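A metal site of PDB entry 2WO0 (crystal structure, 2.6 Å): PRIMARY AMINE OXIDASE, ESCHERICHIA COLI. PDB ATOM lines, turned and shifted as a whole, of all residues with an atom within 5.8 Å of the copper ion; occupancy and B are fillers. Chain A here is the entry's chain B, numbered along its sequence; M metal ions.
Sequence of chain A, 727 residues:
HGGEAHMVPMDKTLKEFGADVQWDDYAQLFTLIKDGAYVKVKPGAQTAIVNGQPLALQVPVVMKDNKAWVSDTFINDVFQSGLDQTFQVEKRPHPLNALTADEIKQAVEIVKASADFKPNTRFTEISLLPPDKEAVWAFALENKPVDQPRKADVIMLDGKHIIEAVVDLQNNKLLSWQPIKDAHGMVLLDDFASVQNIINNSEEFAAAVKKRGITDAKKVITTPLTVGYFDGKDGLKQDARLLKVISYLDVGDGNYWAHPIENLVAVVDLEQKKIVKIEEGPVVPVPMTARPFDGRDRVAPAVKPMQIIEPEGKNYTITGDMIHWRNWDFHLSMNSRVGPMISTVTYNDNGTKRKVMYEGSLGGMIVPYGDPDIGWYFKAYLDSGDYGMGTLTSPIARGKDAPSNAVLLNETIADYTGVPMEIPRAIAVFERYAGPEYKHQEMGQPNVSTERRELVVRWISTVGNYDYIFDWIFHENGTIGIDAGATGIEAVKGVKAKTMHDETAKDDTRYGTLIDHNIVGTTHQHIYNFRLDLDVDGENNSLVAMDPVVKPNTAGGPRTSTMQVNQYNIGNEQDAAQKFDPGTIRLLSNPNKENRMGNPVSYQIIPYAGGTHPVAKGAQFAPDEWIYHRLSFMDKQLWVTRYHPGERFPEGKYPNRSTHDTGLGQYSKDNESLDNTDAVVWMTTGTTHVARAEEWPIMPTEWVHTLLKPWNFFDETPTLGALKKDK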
ATOM      1  N   VAL A 367      -7.235   4.311  -2.423  1.00  0.00           N
ATOM      2  CA  VAL A 367      -8.004   4.492  -1.207  1.00  0.00           C
ATOM      3  C   VAL A 367      -7.114   4.976  -0.068  1.00  0.00           C
ATOM      4  O   VAL A 367      -6.557   4.146   0.654  1.00  0.00           O
ATOM      5  CB  VAL A 367      -8.663   3.197  -0.769  1.00  0.00           C
ATOM      6  CG1 VAL A 367      -9.502   3.448   0.431  1.00  0.00           C
ATOM      7  CG2 VAL A 367      -9.525   2.677  -1.881  1.00  0.00           C
ATOM      8  N   TPQ A 466     -10.949  -4.623   1.218  1.00  0.00           N
ATOM      9  CA  TPQ A 466     -12.188  -4.100   0.683  1.00  0.00           C
ATOM     10  CB  TPQ A 466     -11.942  -2.655   0.250  1.00  0.00           C
ATOM     11  C   TPQ A 466     -12.669  -4.947  -0.482  1.00  0.00           C
ATOM     12  O   TPQ A 466     -11.878  -5.724  -1.065  1.00  0.00           O
ATOM     13  C1  TPQ A 466     -12.577  -1.643   1.189  1.00  0.00           C
ATOM     14  C2  TPQ A 466     -11.765  -0.481   1.631  1.00  0.00           C
ATOM     15  O2  TPQ A 466     -10.491  -0.376   1.175  1.00  0.00           O
ATOM     16  C3  TPQ A 466     -12.304   0.465   2.491  1.00  0.00           C
ATOM     17  C4  TPQ A 466     -13.605   0.327   2.948  1.00  0.00           C
ATOM     18  O4  TPQ A 466     -14.144   1.242   3.786  1.00  0.00           O
ATOM     19  C5  TPQ A 466     -14.423  -0.837   2.525  1.00  0.00           C
ATOM     20  O5  TPQ A 466     -15.708  -0.953   2.988  1.00  0.00           O
ATOM     21  C6  TPQ A 466     -13.881  -1.782   1.656  1.00  0.00           C
ATOM     22  N   GLU A 490     -14.267  -2.787   7.086  1.00  0.00           N
ATOM     23  CA  GLU A 490     -13.576  -1.530   7.280  1.00  0.00           C
ATOM     24  C   GLU A 490     -12.224  -1.642   7.938  1.00  0.00           C
ATOM     25  O   GLU A 490     -12.032  -2.446   8.849  1.00  0.00           O
ATOM     26  CB  GLU A 490     -14.434  -0.632   8.140  1.00  0.00           C
ATOM     27  CG  GLU A 490     -15.476   0.073   7.379  1.00  0.00           C
ATOM     28  CD  GLU A 490     -15.352   1.537   7.609  1.00  0.00           C
ATOM     29  OE1 GLU A 490     -14.411   2.178   7.043  1.00  0.00           O
ATOM     30  OE2 GLU A 490     -16.202   2.042   8.391  1.00  0.00           O
ATOM     31  N   HIS A 524     -11.678   8.033   5.006  1.00  0.00           N
ATOM     32  CA  HIS A 524     -10.777   7.770   3.886  1.00  0.00           C
ATOM     33  C   HIS A 524     -11.578   8.069   2.653  1.00  0.00           C
ATOM     34  O   HIS A 524     -12.749   8.367   2.762  1.00  0.00           O
ATOM     35  CB  HIS A 524     -10.360   6.316   3.893  1.00  0.00           C
ATOM     36  CG  HIS A 524     -11.516   5.372   3.978  1.00  0.00           C
ATOM     37  ND1 HIS A 524     -12.203   5.141   5.156  1.00  0.00           N
ATOM     38  CD2 HIS A 524     -12.142   4.634   3.037  1.00  0.00           C
ATOM     39  CE1 HIS A 524     -13.190   4.284   4.940  1.00  0.00           C
ATOM     40  NE2 HIS A 524     -13.169   3.960   3.661  1.00  0.00           N
ATOM     41  N   HIS A 526     -12.358   6.899  -1.661  1.00  0.00           N
ATOM     42  CA  HIS A 526     -12.280   5.833  -2.647  1.00  0.00           C
ATOM     43  C   HIS A 526     -12.288   6.556  -3.936  1.00  0.00           C
ATOM     44  O   HIS A 526     -13.310   7.111  -4.324  1.00  0.00           O
ATOM     45  CB  HIS A 526     -13.535   4.945  -2.649  1.00  0.00           C
ATOM     46  CG  HIS A 526     -13.728   4.142  -1.390  1.00  0.00           C
ATOM     47  ND1 HIS A 526     -13.164   2.901  -1.205  1.00  0.00           N
ATOM     48  CD2 HIS A 526     -14.483   4.386  -0.292  1.00  0.00           C
ATOM     49  CE1 HIS A 526     -13.552   2.412  -0.049  1.00  0.00           C
ATOM     50  NE2 HIS A 526     -14.351   3.300   0.537  1.00  0.00           N
ATOM     51  N   HIS A 613     -22.504   7.454  -1.285  1.00  0.00           N
ATOM     52  CA  HIS A 613     -21.686   8.038  -0.203  1.00  0.00           C
ATOM     53  C   HIS A 613     -21.522   9.521  -0.555  1.00  0.00           C
ATOM     54  O   HIS A 613     -21.875   9.917  -1.645  1.00  0.00           O
ATOM     55  CB  HIS A 613     -20.285   7.400  -0.169  1.00  0.00           C
ATOM     56  CG  HIS A 613     -20.127   6.277   0.810  1.00  0.00           C
ATOM     57  ND1 HIS A 613     -21.007   6.058   1.851  1.00  0.00           N
ATOM     58  CD2 HIS A 613     -19.160   5.341   0.936  1.00  0.00           C
ATOM     59  CE1 HIS A 613     -20.596   5.024   2.563  1.00  0.00           C
ATOM     60  NE2 HIS A 613     -19.471   4.570   2.039  1.00  0.00           N
ATOM     61  N   THR A 687     -15.602   8.854  -3.528  1.00  0.00           N
ATOM     62  CA  THR A 687     -16.445   9.166  -2.420  1.00  0.00           C
ATOM     63  C   THR A 687     -15.529   9.623  -1.317  1.00  0.00           C
ATOM     64  O   THR A 687     -14.328   9.543  -1.427  1.00  0.00           O
ATOM     65  CB  THR A 687     -17.189   7.929  -1.972  1.00  0.00           C
ATOM     66  OG1 THR A 687     -16.248   6.906  -1.639  1.00  0.00           O
ATOM     67  CG2 THR A 687     -18.068   7.437  -3.108  1.00  0.00           C
ATOM     68  N   HIS A 689     -15.522   8.837   2.685  1.00  0.00           N
ATOM     69  CA  HIS A 689     -16.229   7.897   3.501  1.00  0.00           C
ATOM     70  C   HIS A 689     -16.094   8.163   4.999  1.00  0.00           C
ATOM     71  O   HIS A 689     -15.092   7.836   5.631  1.00  0.00           O
ATOM     72  CB  HIS A 689     -15.857   6.478   3.102  1.00  0.00           C
ATOM     73  CG  HIS A 689     -16.614   5.429   3.857  1.00  0.00           C
ATOM     74  ND1 HIS A 689     -16.366   4.072   3.707  1.00  0.00           N
ATOM     75  CD2 HIS A 689     -17.576   5.532   4.796  1.00  0.00           C
ATOM     76  CE1 HIS A 689     -17.161   3.392   4.510  1.00  0.00           C
ATOM     77  NE2 HIS A 689     -17.903   4.247   5.173  1.00  0.00           N
ATOM     78  N   MET A 699     -19.802  -3.820   5.488  1.00  0.00           N
ATOM     79  CA  MET A 699     -20.395  -2.643   4.856  1.00  0.00           C
ATOM     80  C   MET A 699     -21.346  -2.984   3.707  1.00  0.00           C
ATOM     81  O   MET A 699     -20.970  -3.620   2.743  1.00  0.00           O
ATOM     82  CB  MET A 699     -19.317  -1.658   4.366  1.00  0.00           C
ATOM     83  CG  MET A 699     -19.890  -0.396   3.660  1.00  0.00           C
ATOM     84  SD  MET A 699     -18.706   0.717   2.884  1.00  0.00           S
ATOM     85  CE  MET A 699     -18.339  -0.161   1.385  1.00  0.00           C
HETATM   86 CU    CU M   1     -14.686   3.139   2.390  1.00  0.00          CU
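The copper ion is bound by a ring nitrogen (NE2) of His 526 (1.9 Å), a ring nitrogen (NE2) of His 524 (2.1 Å), a ring nitrogen (ND1) of His 689 (2.3 Å) and O4 of TPQ 466 (2.4 Å). The copper ion has four donor atoms within binding distance.
Within 4 Å of the copper ion: TPQ 466, His 524, His 526 and His 689.
The side-chain carboxylate (OE1) of Glu 490 sits close to O4 of TPQ 466, at 3.4 Å. O of His 526 lies within hydrogen-bond range of N of Thr 687, at 3.0 Å.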
